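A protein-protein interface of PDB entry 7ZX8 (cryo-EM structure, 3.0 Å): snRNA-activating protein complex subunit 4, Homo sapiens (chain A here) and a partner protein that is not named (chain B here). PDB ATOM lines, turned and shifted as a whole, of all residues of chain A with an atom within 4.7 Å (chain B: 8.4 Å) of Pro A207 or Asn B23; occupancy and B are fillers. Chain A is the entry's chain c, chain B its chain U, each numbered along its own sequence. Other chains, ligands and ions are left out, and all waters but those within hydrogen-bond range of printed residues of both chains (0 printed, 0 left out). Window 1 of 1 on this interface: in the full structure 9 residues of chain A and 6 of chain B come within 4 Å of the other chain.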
ATOM      1  N   ARG A 203      18.144  30.626  -8.477  1.00  0.00           N
ATOM      2  CA  ARG A 203      18.546  29.683  -7.442  1.00  0.00           C
ATOM      3  C   ARG A 203      18.522  30.338  -6.070  1.00  0.00           C
ATOM      4  O   ARG A 203      18.210  29.680  -5.070  1.00  0.00           O
ATOM      5  CB  ARG A 203      19.934  29.121  -7.737  1.00  0.00           C
ATOM      6  CG  ARG A 203      19.927  27.783  -8.450  1.00  0.00           C
ATOM      7  CD  ARG A 203      21.279  27.493  -9.071  1.00  0.00           C
ATOM      8  NE  ARG A 203      22.363  28.154  -8.349  1.00  0.00           N
ATOM      9  CZ  ARG A 203      22.964  27.649  -7.279  1.00  0.00           C
ATOM     10  NH1 ARG A 203      22.589  26.473  -6.799  1.00  0.00           N
ATOM     11  NH2 ARG A 203      23.939  28.322  -6.685  1.00  0.00           N
ATOM     12  N   LEU A 204      18.850  31.625  -5.992  1.00  0.00           N
ATOM     13  CA  LEU A 204      18.790  32.298  -4.702  1.00  0.00           C
ATOM     14  C   LEU A 204      17.352  32.578  -4.289  1.00  0.00           C
ATOM     15  O   LEU A 204      17.045  32.650  -3.093  1.00  0.00           O
ATOM     16  CB  LEU A 204      19.597  33.591  -4.749  1.00  0.00           C
ATOM     17  CG  LEU A 204      21.103  33.387  -4.724  1.00  0.00           C
ATOM     18  CD1 LEU A 204      21.793  34.666  -4.306  1.00  0.00           C
ATOM     19  CD2 LEU A 204      21.462  32.254  -3.786  1.00  0.00           C
ATOM     20  N   LEU A 205      16.458  32.741  -5.260  1.00  0.00           N
ATOM     21  CA  LEU A 205      15.104  33.172  -4.936  1.00  0.00           C
ATOM     22  C   LEU A 205      14.215  31.999  -4.563  1.00  0.00           C
ATOM     23  O   LEU A 205      13.392  32.114  -3.650  1.00  0.00           O
ATOM     24  CB  LEU A 205      14.512  33.945  -6.107  1.00  0.00           C
ATOM     25  CG  LEU A 205      15.006  35.384  -6.148  1.00  0.00           C
ATOM     26  CD1 LEU A 205      14.277  36.175  -7.214  1.00  0.00           C
ATOM     27  CD2 LEU A 205      14.798  35.999  -4.791  1.00  0.00           C
ATOM     28  N   GLN A 206      14.350  30.873  -5.266  1.00  0.00           N
ATOM     29  CA  GLN A 206      13.520  29.712  -4.958  1.00  0.00           C
ATOM     30  C   GLN A 206      13.418  29.395  -3.469  1.00  0.00           C
ATOM     31  O   GLN A 206      12.291  29.167  -2.991  1.00  0.00           O
ATOM     32  CB  GLN A 206      14.036  28.492  -5.728  1.00  0.00           C
ATOM     33  CG  GLN A 206      13.408  28.327  -7.087  1.00  0.00           C
ATOM     34  CD  GLN A 206      11.904  28.364  -7.022  1.00  0.00           C
ATOM     35  OE1 GLN A 206      11.260  29.166  -7.696  1.00  0.00           O
ATOM     36  NE2 GLN A 206      11.329  27.500  -6.198  1.00  0.00           N
ATOM     37  N   PRO A 207      14.505  29.379  -2.686  1.00  0.00           N
ATOM     38  CA  PRO A 207      14.349  29.078  -1.255  1.00  0.00           C
ATOM     39  C   PRO A 207      13.481  30.085  -0.530  1.00  0.00           C
ATOM     40  O   PRO A 207      12.590  29.698   0.235  1.00  0.00           O
ATOM     41  CB  PRO A 207      15.793  29.098  -0.734  1.00  0.00           C
ATOM     42  CG  PRO A 207      16.647  28.980  -1.925  1.00  0.00           C
ATOM     43  CD  PRO A 207      15.912  29.651  -3.020  1.00  0.00           C
ATOM     44  N   LYS A 208      13.725  31.377  -0.746  1.00  0.00           N
ATOM     45  CA  LYS A 208      12.951  32.395  -0.051  1.00  0.00           C
ATOM     46  C   LYS A 208      11.499  32.383  -0.498  1.00  0.00           C
ATOM     47  O   LYS A 208      10.594  32.606   0.309  1.00  0.00           O
ATOM     48  CB  LYS A 208      13.567  33.771  -0.274  1.00  0.00           C
ATOM     49  CG  LYS A 208      14.486  34.211   0.844  1.00  0.00           C
ATOM     50  CD  LYS A 208      15.683  33.295   0.962  1.00  0.00           C
ATOM     51  CE  LYS A 208      16.584  33.717   2.102  1.00  0.00           C
ATOM     52  NZ  LYS A 208      17.656  32.719   2.335  1.00  0.00           N
ATOM     53  N   LEU A 209      11.260  32.129  -1.783  1.00  0.00           N
ATOM     54  CA  LEU A 209       9.888  32.021  -2.256  1.00  0.00           C
ATOM     55  C   LEU A 209       9.157  30.881  -1.566  1.00  0.00           C
ATOM     56  O   LEU A 209       8.012  31.045  -1.127  1.00  0.00           O
ATOM     57  CB  LEU A 209       9.860  31.835  -3.771  1.00  0.00           C
ATOM     58  CG  LEU A 209       9.771  33.122  -4.585  1.00  0.00           C
ATOM     59  CD1 LEU A 209       8.454  33.807  -4.287  1.00  0.00           C
ATOM     60  CD2 LEU A 209      10.928  34.058  -4.305  1.00  0.00           C
ATOM     61  N   LEU A 210       9.799  29.717  -1.461  1.00  0.00           N
ATOM     62  CA  LEU A 210       9.141  28.610  -0.773  1.00  0.00           C
ATOM     63  C   LEU A 210       8.938  28.920   0.700  1.00  0.00           C
ATOM     64  O   LEU A 210       7.901  28.569   1.273  1.00  0.00           O
ATOM     65  CB  LEU A 210       9.934  27.321  -0.952  1.00  0.00           C
ATOM     66  CG  LEU A 210       9.472  26.471  -2.132  1.00  0.00           C
ATOM     67  CD1 LEU A 210       8.055  25.990  -1.884  1.00  0.00           C
ATOM     68  CD2 LEU A 210       9.542  27.234  -3.441  1.00  0.00           C
ATOM     69  N   LYS A 211       9.910  29.582   1.326  1.00  0.00           N
ATOM     70  CA  LYS A 211       9.766  29.964   2.727  1.00  0.00           C
ATOM     71  C   LYS A 211       8.561  30.873   2.919  1.00  0.00           C
ATOM     72  O   LYS A 211       7.749  30.673   3.833  1.00  0.00           O
ATOM     73  CB  LYS A 211      11.043  30.649   3.199  1.00  0.00           C
ATOM     74  CG  LYS A 211      10.903  31.426   4.487  1.00  0.00           C
ATOM     75  CD  LYS A 211      12.274  31.821   5.001  1.00  0.00           C
ATOM     76  CE  LYS A 211      12.199  32.426   6.388  1.00  0.00           C
ATOM     77  NZ  LYS A 211      11.516  33.743   6.381  1.00  0.00           N
ATOM     78  N   SER B  16      20.874  16.861  -9.949  1.00  0.00           N
ATOM     79  CA  SER B  16      20.278  18.183 -10.048  1.00  0.00           C
ATOM     80  C   SER B  16      18.966  18.297  -9.287  1.00  0.00           C
ATOM     81  O   SER B  16      18.797  19.244  -8.517  1.00  0.00           O
ATOM     82  CB  SER B  16      20.041  18.548 -11.511  1.00  0.00           C
ATOM     83  OG  SER B  16      19.026  19.529 -11.626  1.00  0.00           O
ATOM     84  N   VAL B  17      18.043  17.365  -9.491  1.00  0.00           N
ATOM     85  CA  VAL B  17      16.767  17.367  -8.786  1.00  0.00           C
ATOM     86  C   VAL B  17      16.965  17.302  -7.280  1.00  0.00           C
ATOM     87  O   VAL B  17      16.267  17.982  -6.527  1.00  0.00           O
ATOM     88  CB  VAL B  17      15.896  16.204  -9.288  1.00  0.00           C
ATOM     89  CG1 VAL B  17      14.808  15.888  -8.294  1.00  0.00           C
ATOM     90  CG2 VAL B  17      15.280  16.556 -10.616  1.00  0.00           C
ATOM     91  N   ILE B  18      17.911  16.487  -6.824  1.00  0.00           N
ATOM     92  CA  ILE B  18      18.138  16.348  -5.390  1.00  0.00           C
ATOM     93  C   ILE B  18      18.649  17.655  -4.811  1.00  0.00           C
ATOM     94  O   ILE B  18      18.146  18.141  -3.792  1.00  0.00           O
ATOM     95  CB  ILE B  18      19.103  15.188  -5.112  1.00  0.00           C
ATOM     96  CG1 ILE B  18      18.390  13.857  -5.340  1.00  0.00           C
ATOM     97  CG2 ILE B  18      19.637  15.266  -3.705  1.00  0.00           C
ATOM     98  CD1 ILE B  18      19.266  12.661  -5.152  1.00  0.00           C
ATOM     99  N   GLU B  19      19.660  18.247  -5.451  1.00  0.00           N
ATOM    100  CA  GLU B  19      20.137  19.548  -5.003  1.00  0.00           C
ATOM    101  C   GLU B  19      19.007  20.566  -4.992  1.00  0.00           C
ATOM    102  O   GLU B  19      18.884  21.368  -4.061  1.00  0.00           O
ATOM    103  CB  GLU B  19      21.283  20.024  -5.893  1.00  0.00           C
ATOM    104  CG  GLU B  19      21.896  21.352  -5.465  1.00  0.00           C
ATOM    105  CD  GLU B  19      21.138  22.562  -6.008  1.00  0.00           C
ATOM    106  OE1 GLU B  19      20.425  22.408  -7.024  1.00  0.00           O
ATOM    107  OE2 GLU B  19      21.263  23.663  -5.426  1.00  0.00           O
ATOM    108  N   ASP B  20      18.162  20.538  -6.023  1.00  0.00           N
ATOM    109  CA  ASP B  20      17.031  21.451  -6.088  1.00  0.00           C
ATOM    110  C   ASP B  20      16.138  21.296  -4.867  1.00  0.00           C
ATOM    111  O   ASP B  20      15.864  22.275  -4.164  1.00  0.00           O
ATOM    112  CB  ASP B  20      16.244  21.192  -7.373  1.00  0.00           C
ATOM    113  CG  ASP B  20      15.127  22.199  -7.601  1.00  0.00           C
ATOM    114  OD1 ASP B  20      14.581  22.211  -8.726  1.00  0.00           O
ATOM    115  OD2 ASP B  20      14.791  22.974  -6.685  1.00  0.00           O
ATOM    116  N   VAL B  21      15.679  20.076  -4.610  1.00  0.00           N
ATOM    117  CA  VAL B  21      14.818  19.827  -3.463  1.00  0.00           C
ATOM    118  C   VAL B  21      15.488  20.297  -2.185  1.00  0.00           C
ATOM    119  O   VAL B  21      14.837  20.859  -1.297  1.00  0.00           O
ATOM    120  CB  VAL B  21      14.447  18.338  -3.387  1.00  0.00           C
ATOM    121  CG1 VAL B  21      13.675  18.059  -2.123  1.00  0.00           C
ATOM    122  CG2 VAL B  21      13.632  17.941  -4.598  1.00  0.00           C
ATOM    123  N   ILE B  22      16.802  20.105  -2.080  1.00  0.00           N
ATOM    124  CA  ILE B  22      17.479  20.467  -0.842  1.00  0.00           C
ATOM    125  C   ILE B  22      17.548  21.971  -0.640  1.00  0.00           C
ATOM    126  O   ILE B  22      17.155  22.463   0.426  1.00  0.00           O
ATOM    127  CB  ILE B  22      18.887  19.865  -0.788  1.00  0.00           C
ATOM    128  CG1 ILE B  22      18.798  18.341  -0.794  1.00  0.00           C
ATOM    129  CG2 ILE B  22      19.638  20.378   0.425  1.00  0.00           C
ATOM    130  CD1 ILE B  22      17.975  17.777   0.332  1.00  0.00           C
ATOM    131  N   ASN B  23      18.030  22.725  -1.624  1.00  0.00           N
ATOM    132  CA  ASN B  23      18.068  24.171  -1.450  1.00  0.00           C
ATOM    133  C   ASN B  23      16.675  24.788  -1.427  1.00  0.00           C
ATOM    134  O   ASN B  23      16.515  25.931  -1.000  1.00  0.00           O
ATOM    135  CB  ASN B  23      18.922  24.825  -2.539  1.00  0.00           C
ATOM    136  CG  ASN B  23      20.403  24.716  -2.256  1.00  0.00           C
ATOM    137  OD1 ASN B  23      20.834  24.857  -1.106  1.00  0.00           O
ATOM    138  ND2 ASN B  23      21.196  24.480  -3.298  1.00  0.00           N
ATOM    139  N   ASP B  24      15.656  24.054  -1.872  1.00  0.00           N
ATOM    140  CA  ASP B  24      14.300  24.574  -1.736  1.00  0.00           C
ATOM    141  C   ASP B  24      13.781  24.380  -0.320  1.00  0.00           C
ATOM    142  O   ASP B  24      13.331  25.336   0.320  1.00  0.00           O
ATOM    143  CB  ASP B  24      13.374  23.908  -2.750  1.00  0.00           C
ATOM    144  CG  ASP B  24      13.639  24.369  -4.167  1.00  0.00           C
ATOM    145  OD1 ASP B  24      14.786  24.774  -4.448  1.00  0.00           O
ATOM    146  OD2 ASP B  24      12.705  24.329  -4.998  1.00  0.00           O
ATOM    147  N   VAL B  25      13.853  23.156   0.197  1.00  0.00           N
ATOM    148  CA  VAL B  25      13.306  22.899   1.520  1.00  0.00           C
ATOM    149  C   VAL B  25      14.251  23.327   2.631  1.00  0.00           C
ATOM    150  O   VAL B  25      13.922  23.144   3.808  1.00  0.00           O
ATOM    151  CB  VAL B  25      12.957  21.414   1.689  1.00  0.00           C
ATOM    152  CG1 VAL B  25      12.126  20.941   0.517  1.00  0.00           C
ATOM    153  CG2 VAL B  25      14.214  20.595   1.821  1.00  0.00           C
ATOM    154  N   ARG B  26      15.414  23.892   2.302  1.00  0.00           N
ATOM    155  CA  ARG B  26      16.321  24.351   3.350  1.00  0.00           C
ATOM    156  C   ARG B  26      15.662  25.400   4.232  1.00  0.00           C
ATOM    157  O   ARG B  26      15.671  25.284   5.464  1.00  0.00           O
ATOM    158  CB  ARG B  26      17.602  24.908   2.736  1.00  0.00           C
ATOM    159  CG  ARG B  26      18.384  25.789   3.690  1.00  0.00           C
ATOM    160  CD  ARG B  26      19.568  26.436   3.003  1.00  0.00           C
ATOM    161  NE  ARG B  26      20.588  25.458   2.647  1.00  0.00           N
ATOM    162  CZ  ARG B  26      21.741  25.320   3.292  1.00  0.00           C
ATOM    163  NH1 ARG B  26      22.019  26.103   4.322  1.00  0.00           N
ATOM    164  NH2 ARG B  26      22.615  24.403   2.903  1.00  0.00           N
ATOM    165  N   ASP B  27      15.082  26.435   3.622  1.00  0.00           N
ATOM    166  CA  ASP B  27      14.459  27.489   4.412  1.00  0.00           C
ATOM    167  C   ASP B  27      13.210  26.979   5.118  1.00  0.00           C
ATOM    168  O   ASP B  27      12.913  27.388   6.243  1.00  0.00           O
ATOM    169  CB  ASP B  27      14.126  28.689   3.534  1.00  0.00           C
ATOM    170  CG  ASP B  27      15.346  29.267   2.864  1.00  0.00           C
ATOM    171  OD1 ASP B  27      15.192  30.178   2.026  1.00  0.00           O
ATOM    172  OD2 ASP B  27      16.462  28.794   3.168  1.00  0.00           O
ATOM    173  N   ILE B  28      12.458  26.092   4.469  1.00  0.00           N
ATOM    174  CA  ILE B  28      11.304  25.492   5.129  1.00  0.00           C
ATOM    175  C   ILE B  28      11.735  24.776   6.399  1.00  0.00           C
ATOM    176  O   ILE B  28      11.075  24.872   7.441  1.00  0.00           O
ATOM    177  CB  ILE B  28      10.578  24.538   4.166  1.00  0.00           C
ATOM    178  CG1 ILE B  28       9.986  25.322   2.995  1.00  0.00           C
ATOM    179  CG2 ILE B  28       9.500  23.763   4.894  1.00  0.00           C
ATOM    180  CD1 ILE B  28       9.172  24.476   2.051  1.00  0.00           C
ATOM    181  N   PHE B  29      12.861  24.067   6.338  1.00  0.00           N
ATOM    182  CA  PHE B  29      13.300  23.301   7.496  1.00  0.00           C
ATOM    183  C   PHE B  29      13.874  24.216   8.565  1.00  0.00           C
ATOM    184  O   PHE B  29      13.716  23.959   9.763  1.00  0.00           O
ATOM    185  CB  PHE B  29      14.320  22.247   7.075  1.00  0.00           C
ATOM    186  CG  PHE B  29      13.744  21.154   6.225  1.00  0.00           C
ATOM    187  CD1 PHE B  29      12.416  21.183   5.833  1.00  0.00           C
ATOM    188  CD2 PHE B  29      14.525  20.090   5.824  1.00  0.00           C
ATOM    189  CE1 PHE B  29      11.888  20.187   5.051  1.00  0.00           C
ATOM    190  CE2 PHE B  29      13.996  19.085   5.046  1.00  0.00           C
ATOM    191  CZ  PHE B  29      12.678  19.135   4.659  1.00  0.00           C
ATOM    192  N   GLU B  36      19.499  21.674   9.999  1.00  0.00           N
ATOM    193  CA  GLU B  36      20.085  21.292   8.723  1.00  0.00           C
ATOM    194  C   GLU B  36      20.616  19.867   8.746  1.00  0.00           C
ATOM    195  O   GLU B  36      20.663  19.206   7.703  1.00  0.00           O
ATOM    196  CB  GLU B  36      21.201  22.268   8.349  1.00  0.00           C
ATOM    197  CG  GLU B  36      21.407  22.432   6.854  1.00  0.00           C
ATOM    198  CD  GLU B  36      22.133  21.261   6.233  1.00  0.00           C
ATOM    199  OE1 GLU B  36      23.031  20.705   6.898  1.00  0.00           O
ATOM    200  OE2 GLU B  36      21.803  20.888   5.088  1.00  0.00           O
ATOM    201  N   LEU B  39      18.135  17.538   7.577  1.00  0.00           N
ATOM    202  CA  LEU B  39      17.965  17.711   6.142  1.00  0.00           C
ATOM    203  C   LEU B  39      19.033  16.956   5.363  1.00  0.00           C
ATOM    204  O   LEU B  39      18.726  16.260   4.387  1.00  0.00           O
ATOM    205  CB  LEU B  39      17.992  19.194   5.799  1.00  0.00           C
ATOM    206  CG  LEU B  39      18.290  19.548   4.350  1.00  0.00           C
ATOM    207  CD1 LEU B  39      17.118  19.150   3.483  1.00  0.00           C
ATOM    208  CD2 LEU B  39      18.579  21.030   4.222  1.00  0.00           C
ATOM    209  N   LYS B  43      18.764  13.873   2.712  1.00  0.00           N
ATOM    210  CA  LYS B  43      19.446  13.853   1.423  1.00  0.00           C
ATOM    211  C   LYS B  43      20.220  12.556   1.238  1.00  0.00           C
ATOM    212  O   LYS B  43      20.098  11.881   0.206  1.00  0.00           O
ATOM    213  CB  LYS B  43      20.381  15.054   1.322  1.00  0.00           C
ATOM    214  CG  LYS B  43      21.115  15.169   0.006  1.00  0.00           C
ATOM    215  CD  LYS B  43      22.185  16.241   0.086  1.00  0.00           C
ATOM    216  CE  LYS B  43      22.645  16.673  -1.294  1.00  0.00           C
ATOM    217  NZ  LYS B  43      23.102  15.522  -2.121  1.00  0.00           N
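NE2 of Gln A206 touches OD2 of Asp B24 (3.7 Å).
Pro A207 touches Asn B23.
Lys A211 touches Asp B27.
Printed residues of chain B within 4 Å of Arg A203: Glu B19 (3.4 Å).
Of the printed residues of chain B, Gln A206 touches Asp B24.
Pro A207 touches two residues of chain B.
Of the printed residues of chain B, Lys A208 touches Asp B27 (3.3 Å).
Printed residues of chain A within 4 Å of Glu B19: Arg A203.
Of the printed residues of chain A, Asn B23 touches Pro A207.
The nearest residue of chain B that does not touch Pro A207 is Asp B24 (4.2 Å).
The nearest residue of chain A that does not touch Asn B23 is Arg A203 (4.3 Å).
The side-chain carboxylate (OD1) of Asp B24 lies close to the backbone carbonyl oxygen (O) of Asp B20.
Hydrophobic or aromatic side chains of chain A within 4 Å of the printed part of chain B: Pro A207.
NH1 of Arg A203 lies within salt-bridge range of OE2 of Glu B19 (3.4 Å).
OD1 of Asp B27 is in salt-bridge range of NZ of Lys A208, at 3.6 Å.
OD1 of Asp B27 sits close to O of Pro A207.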
